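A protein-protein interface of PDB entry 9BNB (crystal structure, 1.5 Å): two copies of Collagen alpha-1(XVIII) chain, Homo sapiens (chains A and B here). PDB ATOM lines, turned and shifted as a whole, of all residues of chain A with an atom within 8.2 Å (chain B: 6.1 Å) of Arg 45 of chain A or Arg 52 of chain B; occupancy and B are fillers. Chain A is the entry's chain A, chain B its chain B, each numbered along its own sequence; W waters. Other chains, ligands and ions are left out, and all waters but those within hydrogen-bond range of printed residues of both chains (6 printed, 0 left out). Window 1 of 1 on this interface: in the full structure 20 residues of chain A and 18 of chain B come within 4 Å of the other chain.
The guanidinium group (NH2) of Arg 52 of chain B is in hydrogen-bond range of the backbone carbonyl oxygen (O) of Gln 41 of chain A (3.0 Å). The guanidinium group (NH2) of Arg 52 of chain B is in hydrogen-bond range of the backbone carbonyl oxygen (O) of Asn 42 of chain A. The backbone carbonyl oxygen of Thr 53 of chain B is in hydrogen-bond range of the backbone NH of Phe 44 of chain A, 2.9 Å away. The guanidinium group (NH1) of Arg 45 of chain A lies within hydrogen-bond range of the backbone carbonyl oxygen (O) of Gln 33 of chain B (3.5 Å). NH1 of Arg 45 of chain A sits at hydrogen-bond distance from O of Glu 34 of chain B, 2.7 Å away. NH2 of Arg 45 of chain A is in hydrogen-bond range of O of Leu 49 of chain B (3.4 Å). O of Glu 50 of chain B sits at hydrogen-bond distance from NE of Arg 45 of chain A. The backbone carbonyl oxygen (O) of Lys 46 of chain A sits at hydrogen-bond distance from the backbone NH (N) of Glu 50 of chain B, 2.9 Å away.
The backbone carbonyl oxygen of Leu 36 of chain A lies within hydrogen-bond range of the backbone NH of Val 47 of chain A. The backbone NH of Val 38 of chain A is in hydrogen-bond range of the backbone carbonyl oxygen of Arg 45 of chain A, 2.8 Å away. The backbone carbonyl oxygen (O) of Gly 43 of chain A sits at hydrogen-bond distance from the guanidinium group (NH1) of Arg 39 of chain A, 3.2 Å away.
Leu 49 of chain B touches Val 38 of chain A (CD2 to CG2, 3.9 Å). CB of Val 40 of chain A touches OE2 of Glu 34 of chain B, at 3.6 Å. O of Asn 42 of chain A touches CA of Pro 54 of chain B, at 3.9 Å. Arg 52 of chain B touches Gly 43 of chain A (NH2 to N, 3.8 Å). O of Thr 53 of chain B touches CA of Gly 43 of chain A (3.3 Å). O of Phe 44 of chain A touches CA of Arg 52 of chain B (3.3 Å). Phe 44 of chain A touches Pro 54 of chain B. Arg 52 of chain B touches Arg 45 of chain A. Lys 46 of chain A touches Leu 49 of chain B (O to CA, 3.4 Å). Gln 48 of chain A touches Leu 49 of chain B (NE2 to O, 3.7 Å).
Of the printed residues of chain B, Phe 44 of chain A touches Arg 52, Thr 53 and Pro 54. Of chain B, only Gln 33, Glu 34, Leu 49, Glu 50 and Arg 52 come within 4 Å of Arg 45 of chain A. Of the printed residues of chain B, Val 47 of chain A touches Leu 49. Of the printed residues of chain B, Gln 48 of chain A touches Leu 49 (3.7 Å). Of the printed residues of chain A, Glu 34 of chain B touches Val 40 (3.6 Å) and Arg 45 (2.7 Å). Of the printed residues of chain A, Glu 50 of chain B touches Arg 45 and Lys 46. No residue of chain A comes within 4 Å of Ala 51 of chain B. Arg 52 of chain B touches just these residues of chain A: Val 40, Gln 41, Asn 42, Gly 43, Phe 44 and Arg 45. Thr 53 of chain B touches just these residues of chain A: Gly 43 and Phe 44. The nearest residue of chain B that does not touch Arg 45 of chain A is Ala 51 of chain B (4.1 Å). The nearest residue of chain A that does not touch Arg 52 of chain B is Lys 46 of chain A (6.3 Å).
Of the 16 printed residues of chain A, 10 touch a printed residue of chain B. Hydrophobic or aromatic side chains of chain A that line the printed part of chain B: Val 38, Val 40, Phe 44 and Val 47. Among the printed residues, 20 pairs touch across the chains. Among the printed residues, no Asp or Glu carboxylate lies within 4 Å of a Lys or Arg side-chain nitrogen of the other chain.
No position is printed for both chains. Of the 20 pairs that touch across the chains among the printed residues, none has its exchanged pair printed and touching as well.
Water W5 lies within hydrogen-bond range of the guanidinium group of Arg 52 of chain B (2.5 Å), the side-chain carboxylate of Glu 34 of chain B (2.6 Å) and the backbone carbonyl oxygen of Gln 41 of chain A (2.8 Å). Water W6 lies within hydrogen-bond range of the backbone carbonyl oxygen of Asn 42 of chain A (2.6 Å) and the backbone carbonyl oxygen of Pro 54 of chain B (2.6 Å). Water W4 bridges O of Leu 49 of chain B (2.6 Å) and NE2 of Gln 48 of chain A (2.9 Å). Water W1 lies within hydrogen-bond range of the guanidinium group of Arg 52 of chain B and the backbone carbonyl oxygen of Asn 42 of chain A. Water W2 bridges the backbone carbonyl oxygen (O) of Ala 51 of chain B (2.8 Å) and the backbone NH (N) of Lys 46 of chain A (3.0 Å). Water W3 bridges OE1 of Glu 34 of chain B (2.9 Å) and NH1 of Arg 45 of chain A (3.3 Å).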
ATOM      1  N   TRP A  26      22.531   3.015   4.960  1.00  0.00           N
ATOM      2  CA  TRP A  26      23.750   3.496   5.573  1.00  0.00           C
ATOM      3  C   TRP A  26      24.628   2.331   5.975  1.00  0.00           C
ATOM      4  O   TRP A  26      24.143   1.241   6.226  1.00  0.00           O
ATOM      5  CB  TRP A  26      23.436   4.333   6.803  1.00  0.00           C
ATOM      6  CG  TRP A  26      23.007   5.720   6.483  1.00  0.00           C
ATOM      7  CD1 TRP A  26      21.826   6.102   5.934  1.00  0.00           C
ATOM      8  CD2 TRP A  26      23.765   6.920   6.664  1.00  0.00           C
ATOM      9  NE1 TRP A  26      21.796   7.452   5.757  1.00  0.00           N
ATOM     10  CE2 TRP A  26      22.975   7.976   6.202  1.00  0.00           C
ATOM     11  CE3 TRP A  26      25.039   7.201   7.166  1.00  0.00           C
ATOM     12  CZ2 TRP A  26      23.419   9.300   6.241  1.00  0.00           C
ATOM     13  CZ3 TRP A  26      25.476   8.512   7.188  1.00  0.00           C
ATOM     14  CH2 TRP A  26      24.666   9.543   6.731  1.00  0.00           C
ATOM     15  N   LEU A  27      25.923   2.547   6.032  1.00  0.00           N
ATOM     16  CA  LEU A  27      26.866   1.560   6.546  1.00  0.00           C
ATOM     17  C   LEU A  27      27.209   1.842   8.000  1.00  0.00           C
ATOM     18  O   LEU A  27      27.253   3.010   8.432  1.00  0.00           O
ATOM     19  CB  LEU A  27      28.153   1.549   5.723  1.00  0.00           C
ATOM     20  CG  LEU A  27      28.071   0.739   4.426  1.00  0.00           C
ATOM     21  CD1 LEU A  27      27.013   1.259   3.527  1.00  0.00           C
ATOM     22  CD2 LEU A  27      29.419   0.805   3.727  1.00  0.00           C
ATOM     23  N   ILE A  28      27.470   0.783   8.761  1.00  0.00           N
ATOM     24  CA  ILE A  28      27.674   0.838  10.211  1.00  0.00           C
ATOM     25  C   ILE A  28      28.970   0.122  10.511  1.00  0.00           C
ATOM     26  O   ILE A  28      29.106  -1.072  10.234  1.00  0.00           O
ATOM     27  CB  ILE A  28      26.499   0.189  10.972  1.00  0.00           C
ATOM     28  CG1 ILE A  28      25.208   1.005  10.832  1.00  0.00           C
ATOM     29  CG2 ILE A  28      26.823  -0.023  12.438  1.00  0.00           C
ATOM     30  CD1 ILE A  28      23.950   0.265  11.232  1.00  0.00           C
ATOM     31  N   LEU A  36      31.552  -4.483   9.937  1.00  0.00           N
ATOM     32  CA  LEU A  36      30.920  -3.545   9.021  1.00  0.00           C
ATOM     33  C   LEU A  36      29.595  -4.149   8.569  1.00  0.00           C
ATOM     34  O   LEU A  36      29.567  -5.285   8.086  1.00  0.00           O
ATOM     35  CB  LEU A  36      31.790  -3.242   7.802  1.00  0.00           C
ATOM     36  CG  LEU A  36      31.255  -2.183   6.863  1.00  0.00           C
ATOM     37  CD1 LEU A  36      31.197  -0.736   7.524  1.00  0.00           C
ATOM     38  CD2 LEU A  36      32.046  -2.126   5.584  1.00  0.00           C
ATOM     39  N   TYR A  37      28.506  -3.399   8.713  1.00  0.00           N
ATOM     40  CA  TYR A  37      27.165  -3.815   8.326  1.00  0.00           C
ATOM     41  C   TYR A  37      26.517  -2.796   7.396  1.00  0.00           C
ATOM     42  O   TYR A  37      26.808  -1.591   7.463  1.00  0.00           O
ATOM     43  CB  TYR A  37      26.233  -3.971   9.583  1.00  0.00           C
ATOM     44  CG  TYR A  37      26.761  -4.893  10.649  1.00  0.00           C
ATOM     45  CD1 TYR A  37      27.565  -4.407  11.672  1.00  0.00           C
ATOM     46  CD2 TYR A  37      26.480  -6.245  10.642  1.00  0.00           C
ATOM     47  CE1 TYR A  37      28.067  -5.219  12.665  1.00  0.00           C
ATOM     48  CE2 TYR A  37      27.010  -7.081  11.634  1.00  0.00           C
ATOM     49  CZ  TYR A  37      27.812  -6.543  12.643  1.00  0.00           C
ATOM     50  OH  TYR A  37      28.329  -7.320  13.664  1.00  0.00           O
ATOM     51  N   VAL A  38      25.639  -3.284   6.548  1.00  0.00           N
ATOM     52  CA  VAL A  38      24.690  -2.450   5.843  1.00  0.00           C
ATOM     53  C   VAL A  38      23.409  -2.450   6.656  1.00  0.00           C
ATOM     54  O   VAL A  38      22.896  -3.510   7.023  1.00  0.00           O
ATOM     55  CB  VAL A  38      24.431  -2.942   4.415  1.00  0.00           C
ATOM     56  CG1 VAL A  38      23.402  -2.038   3.763  1.00  0.00           C
ATOM     57  CG2 VAL A  38      25.694  -3.050   3.631  1.00  0.00           C
ATOM     58  N   ARG A  39      22.939  -1.255   7.010  1.00  0.00           N
ATOM     59  CA  ARG A  39      21.653  -1.109   7.655  1.00  0.00           C
ATOM     60  C   ARG A  39      20.540  -1.369   6.643  1.00  0.00           C
ATOM     61  O   ARG A  39      20.461  -0.696   5.613  1.00  0.00           O
ATOM     62  CB  ARG A  39      21.503   0.295   8.268  1.00  0.00           C
ATOM     63  CG  ARG A  39      20.120   0.594   8.909  1.00  0.00           C
ATOM     64  CD  ARG A  39      19.882  -0.279  10.096  1.00  0.00           C
ATOM     65  NE  ARG A  39      18.707   0.148  10.857  1.00  0.00           N
ATOM     66  CZ  ARG A  39      18.132  -0.619  11.765  1.00  0.00           C
ATOM     67  NH1 ARG A  39      18.523  -1.865  11.949  1.00  0.00           N
ATOM     68  NH2 ARG A  39      17.164  -0.109  12.534  1.00  0.00           N
ATOM     69  N   VAL A  40      19.652  -2.307   6.967  1.00  0.00           N
ATOM     70  CA  VAL A  40      18.511  -2.579   6.103  1.00  0.00           C
ATOM     71  C   VAL A  40      17.286  -2.377   6.965  1.00  0.00           C
ATOM     72  O   VAL A  40      17.392  -2.081   8.163  1.00  0.00           O
ATOM     73  CB  VAL A  40      18.580  -3.971   5.417  1.00  0.00           C
ATOM     74  CG1 VAL A  40      19.761  -3.956   4.439  1.00  0.00           C
ATOM     75  CG2 VAL A  40      18.709  -5.126   6.389  1.00  0.00           C
ATOM     76  N   GLN A  41      16.123  -2.481   6.359  1.00  0.00           N
ATOM     77  CA  GLN A  41      14.904  -2.235   7.101  1.00  0.00           C
ATOM     78  C   GLN A  41      14.814  -3.191   8.297  1.00  0.00           C
ATOM     79  O   GLN A  41      14.802  -4.411   8.140  1.00  0.00           O
ATOM     80  CB  GLN A  41      13.697  -2.388   6.179  1.00  0.00           C
ATOM     81  CG  GLN A  41      12.366  -1.928   6.833  1.00  0.00           C
ATOM     82  CD  GLN A  41      11.116  -2.201   5.981  1.00  0.00           C
ATOM     83  OE1 GLN A  41      10.295  -1.304   5.753  1.00  0.00           O
ATOM     84  NE2 GLN A  41      10.952  -3.450   5.536  1.00  0.00           N
ATOM     85  N   ASN A  42      14.823  -2.612   9.496  1.00  0.00           N
ATOM     86  CA  ASN A  42      14.745  -3.325  10.790  1.00  0.00           C
ATOM     87  C   ASN A  42      15.783  -4.441  10.934  1.00  0.00           C
ATOM     88  O   ASN A  42      15.533  -5.451  11.595  1.00  0.00           O
ATOM     89  CB  ASN A  42      13.370  -3.940  11.029  1.00  0.00           C
ATOM     90  CG  ASN A  42      12.259  -2.939  10.972  1.00  0.00           C
ATOM     91  OD1 ASN A  42      12.325  -1.894  11.619  1.00  0.00           O
ATOM     92  ND2 ASN A  42      11.180  -3.290  10.258  1.00  0.00           N
ATOM     93  N   GLY A  43      16.951  -4.295  10.330  1.00  0.00           N
ATOM     94  CA  GLY A  43      17.935  -5.339  10.458  1.00  0.00           C
ATOM     95  C   GLY A  43      19.260  -4.935   9.836  1.00  0.00           C
ATOM     96  O   GLY A  43      19.542  -3.755   9.621  1.00  0.00           O
ATOM     97  N   PHE A  44      20.063  -5.957   9.537  1.00  0.00           N
ATOM     98  CA  PHE A  44      21.444  -5.768   9.128  1.00  0.00           C
ATOM     99  C   PHE A  44      21.805  -6.818   8.113  1.00  0.00           C
ATOM    100  O   PHE A  44      21.304  -7.943   8.167  1.00  0.00           O
ATOM    101  CB  PHE A  44      22.426  -5.918  10.326  1.00  0.00           C
ATOM    102  CG  PHE A  44      22.062  -5.073  11.481  1.00  0.00           C
ATOM    103  CD1 PHE A  44      21.155  -5.526  12.414  1.00  0.00           C
ATOM    104  CD2 PHE A  44      22.625  -3.832  11.635  1.00  0.00           C
ATOM    105  CE1 PHE A  44      20.775  -4.738  13.482  1.00  0.00           C
ATOM    106  CE2 PHE A  44      22.227  -3.022  12.720  1.00  0.00           C
ATOM    107  CZ  PHE A  44      21.303  -3.509  13.617  1.00  0.00           C
ATOM    108  N   ARG A  45      22.729  -6.457   7.241  1.00  0.00           N
ATOM    109  CA  ARG A  45      23.450  -7.400   6.386  1.00  0.00           C
ATOM    110  C   ARG A  45      24.932  -7.189   6.630  1.00  0.00           C
ATOM    111  O   ARG A  45      25.458  -6.101   6.392  1.00  0.00           O
ATOM    112  CB  ARG A  45      23.127  -7.202   4.900  1.00  0.00           C
ATOM    113  CG  ARG A  45      21.696  -7.598   4.575  1.00  0.00           C
ATOM    114  CD  ARG A  45      21.489  -7.716   3.104  1.00  0.00           C
ATOM    115  NE  ARG A  45      22.083  -8.950   2.606  1.00  0.00           N
ATOM    116  CZ  ARG A  45      22.073  -9.336   1.339  1.00  0.00           C
ATOM    117  NH1 ARG A  45      21.503  -8.606   0.387  1.00  0.00           N
ATOM    118  NH2 ARG A  45      22.633 -10.497   1.020  1.00  0.00           N
ATOM    119  N   LYS A  46      25.601  -8.195   7.170  1.00  0.00           N
ATOM    120  CA  LYS A  46      27.018  -8.075   7.474  1.00  0.00           C
ATOM    121  C   LYS A  46      27.853  -8.144   6.209  1.00  0.00           C
ATOM    122  O   LYS A  46      27.652  -9.009   5.365  1.00  0.00           O
ATOM    123  CB  LYS A  46      27.404  -9.161   8.463  1.00  0.00           C
ATOM    124  CG  LYS A  46      28.851  -9.103   8.901  1.00  0.00           C
ATOM    125  CD  LYS A  46      29.117 -10.284   9.827  1.00  0.00           C
ATOM    126  CE  LYS A  46      30.209  -9.944  10.826  1.00  0.00           C
ATOM    127  NZ  LYS A  46      30.478 -11.082  11.753  1.00  0.00           N
ATOM    128  N   VAL A  47      28.736  -7.176   6.060  1.00  0.00           N
ATOM    129  CA  VAL A  47      29.710  -7.191   4.972  1.00  0.00           C
ATOM    130  C   VAL A  47      30.733  -8.298   5.196  1.00  0.00           C
ATOM    131  O   VAL A  47      31.292  -8.423   6.285  1.00  0.00           O
ATOM    132  CB  VAL A  47      30.396  -5.816   4.830  1.00  0.00           C
ATOM    133  CG1 VAL A  47      31.345  -5.828   3.632  1.00  0.00           C
ATOM    134  CG2 VAL A  47      29.335  -4.710   4.625  1.00  0.00           C
ATOM    135  N   GLN A  48      30.990  -9.096   4.165  1.00  0.00           N
ATOM    136  CA  GLN A  48      32.055 -10.091   4.233  1.00  0.00           C
ATOM    137  C   GLN A  48      33.431  -9.445   4.155  1.00  0.00           C
ATOM    138  O   GLN A  48      33.767  -8.837   3.145  1.00  0.00           O
ATOM    139  CB  GLN A  48      31.843 -11.125   3.137  1.00  0.00           C
ATOM    140  CG  GLN A  48      30.508 -11.868   3.281  1.00  0.00           C
ATOM    141  CD  GLN A  48      30.354 -13.045   2.334  1.00  0.00           C
ATOM    142  OE1 GLN A  48      31.315 -13.747   2.028  1.00  0.00           O
ATOM    143  NE2 GLN A  48      29.115 -13.289   1.895  1.00  0.00           N
ATOM    144  N   GLN B  33      16.720  -5.215  -3.549  1.00  0.00           N
ATOM    145  CA  GLN B  33      17.398  -6.447  -3.190  1.00  0.00           C
ATOM    146  C   GLN B  33      18.336  -6.295  -2.000  1.00  0.00           C
ATOM    147  O   GLN B  33      19.037  -7.255  -1.670  1.00  0.00           O
ATOM    148  CB  GLN B  33      18.211  -6.946  -4.382  1.00  0.00           C
ATOM    149  CG  GLN B  33      17.366  -7.366  -5.560  1.00  0.00           C
ATOM    150  CD  GLN B  33      17.153  -6.242  -6.540  1.00  0.00           C
ATOM    151  OE1 GLN B  33      17.718  -5.150  -6.410  1.00  0.00           O
ATOM    152  NE2 GLN B  33      16.331  -6.503  -7.545  1.00  0.00           N
ATOM    153  N   GLU B  34      18.396  -5.115  -1.383  1.00  0.00           N
ATOM    154  CA  GLU B  34      19.282  -4.847  -0.244  1.00  0.00           C
ATOM    155  C   GLU B  34      20.735  -5.174  -0.575  1.00  0.00           C
ATOM    156  O   GLU B  34      21.426  -5.881   0.157  1.00  0.00           O
ATOM    157  CB  GLU B  34      18.822  -5.591   1.009  1.00  0.00           C
ATOM    158  CG  GLU B  34      17.361  -5.252   1.417  1.00  0.00           C
ATOM    159  CD  GLU B  34      16.865  -5.968   2.666  1.00  0.00           C
ATOM    160  OE1 GLU B  34      17.353  -7.087   2.927  1.00  0.00           O
ATOM    161  OE2 GLU B  34      15.979  -5.417   3.375  1.00  0.00           O
ATOM    162  N   GLU B  35      21.190  -4.656  -1.699  1.00  0.00           N
ATOM    163  CA  GLU B  35      22.506  -4.959  -2.227  1.00  0.00           C
ATOM    164  C   GLU B  35      23.359  -3.717  -2.238  1.00  0.00           C
ATOM    165  O   GLU B  35      22.864  -2.577  -2.305  1.00  0.00           O
ATOM    166  CB  GLU B  35      22.382  -5.545  -3.614  1.00  0.00           C
ATOM    167  CG  GLU B  35      21.792  -6.944  -3.527  1.00  0.00           C
ATOM    168  CD  GLU B  35      21.693  -7.642  -4.845  1.00  0.00           C
ATOM    169  OE1 GLU B  35      21.647  -6.940  -5.877  1.00  0.00           O
ATOM    170  OE2 GLU B  35      21.599  -8.893  -4.830  1.00  0.00           O
ATOM    171  N   LEU B  49      27.661  -9.718   0.813  1.00  0.00           N
ATOM    172  CA  LEU B  49      26.924  -9.511   2.039  1.00  0.00           C
ATOM    173  C   LEU B  49      26.317 -10.817   2.516  1.00  0.00           C
ATOM    174  O   LEU B  49      25.787 -11.592   1.707  1.00  0.00           O
ATOM    175  CB  LEU B  49      25.782  -8.532   1.815  1.00  0.00           C
ATOM    176  CG  LEU B  49      26.143  -7.176   1.232  1.00  0.00           C
ATOM    177  CD1 LEU B  49      24.854  -6.427   1.010  1.00  0.00           C
ATOM    178  CD2 LEU B  49      26.996  -6.407   2.148  1.00  0.00           C
ATOM    179  N   GLU B  50      26.355 -11.035   3.819  1.00  0.00           N
ATOM    180  CA  GLU B  50      25.541 -12.097   4.393  1.00  0.00           C
ATOM    181  C   GLU B  50      24.057 -11.769   4.383  1.00  0.00           C
ATOM    182  O   GLU B  50      23.617 -10.645   4.145  1.00  0.00           O
ATOM    183  CB  GLU B  50      26.039 -12.477   5.783  1.00  0.00           C
ATOM    184  CG  GLU B  50      27.518 -12.367   5.964  1.00  0.00           C
ATOM    185  CD  GLU B  50      27.988 -13.020   7.231  1.00  0.00           C
ATOM    186  OE1 GLU B  50      27.222 -13.043   8.221  1.00  0.00           O
ATOM    187  OE2 GLU B  50      29.116 -13.567   7.207  1.00  0.00           O
ATOM    188  N   ALA B  51      23.264 -12.814   4.573  1.00  0.00           N
ATOM    189  CA  ALA B  51      21.831 -12.623   4.491  1.00  0.00           C
ATOM    190  C   ALA B  51      21.348 -11.713   5.620  1.00  0.00           C
ATOM    191  O   ALA B  51      21.937 -11.644   6.702  1.00  0.00           O
ATOM    192  CB  ALA B  51      21.109 -13.959   4.539  1.00  0.00           C
ATOM    193  N   ARG B  52      20.268 -10.995   5.339  1.00  0.00           N
ATOM    194  CA  ARG B  52      19.598 -10.156   6.334  1.00  0.00           C
ATOM    195  C   ARG B  52      19.282 -10.918   7.612  1.00  0.00           C
ATOM    196  O   ARG B  52      18.747 -12.026   7.576  1.00  0.00           O
ATOM    197  CB  ARG B  52      18.313  -9.616   5.743  1.00  0.00           C
ATOM    198  CG  ARG B  52      17.678  -8.429   6.435  1.00  0.00           C
ATOM    199  CD  ARG B  52      16.170  -8.690   6.586  1.00  0.00           C
ATOM    200  NE  ARG B  52      15.563  -7.764   7.530  1.00  0.00           N
ATOM    201  CZ  ARG B  52      15.088  -8.057   8.741  1.00  0.00           C
ATOM    202  NH1 ARG B  52      15.179  -9.274   9.265  1.00  0.00           N
ATOM    203  NH2 ARG B  52      14.498  -7.097   9.447  1.00  0.00           N
ATOM    204  N   THR B  53      19.529 -10.269   8.747  1.00  0.00           N
ATOM    205  CA  THR B  53      19.154 -10.748  10.066  1.00  0.00           C
ATOM    206  C   THR B  53      18.685  -9.558  10.880  1.00  0.00           C
ATOM    207  O   THR B  53      19.146  -8.432  10.665  1.00  0.00           O
ATOM    208  CB  THR B  53      20.316 -11.413  10.815  1.00  0.00           C
ATOM    209  OG1 THR B  53      21.474 -10.565  10.761  1.00  0.00           O
ATOM    210  CG2 THR B  53      20.663 -12.754  10.206  1.00  0.00           C
ATOM    211  N   PRO B  54      17.825  -9.781  11.866  1.00  0.00           N
ATOM    212  CA  PRO B  54      17.449  -8.677  12.749  1.00  0.00           C
ATOM    213  C   PRO B  54      18.558  -8.262  13.693  1.00  0.00           C
ATOM    214  O   PRO B  54      18.554  -7.115  14.139  1.00  0.00           O
ATOM    215  CB  PRO B  54      16.224  -9.219  13.509  1.00  0.00           C
ATOM    216  CG  PRO B  54      16.097 -10.662  13.134  1.00  0.00           C
ATOM    217  CD  PRO B  54      17.267 -11.072  12.290  1.00  0.00           C
HETATM  218  O   HOH W   1      12.840  -7.372  11.670  1.00  0.00           O
HETATM  219  O   HOH W   2      24.043 -10.522   8.147  1.00  0.00           O
HETATM  220  O   HOH W   3      18.707  -9.382   1.861  1.00  0.00           O
HETATM  221  O   HOH W   4      26.810 -13.477   0.158  1.00  0.00           O
HETATM  222  O   HOH W   5      15.157  -5.966   5.828  1.00  0.00           O
HETATM  223  O   HOH W   6      16.316  -5.784  14.053  1.00  0.00           O
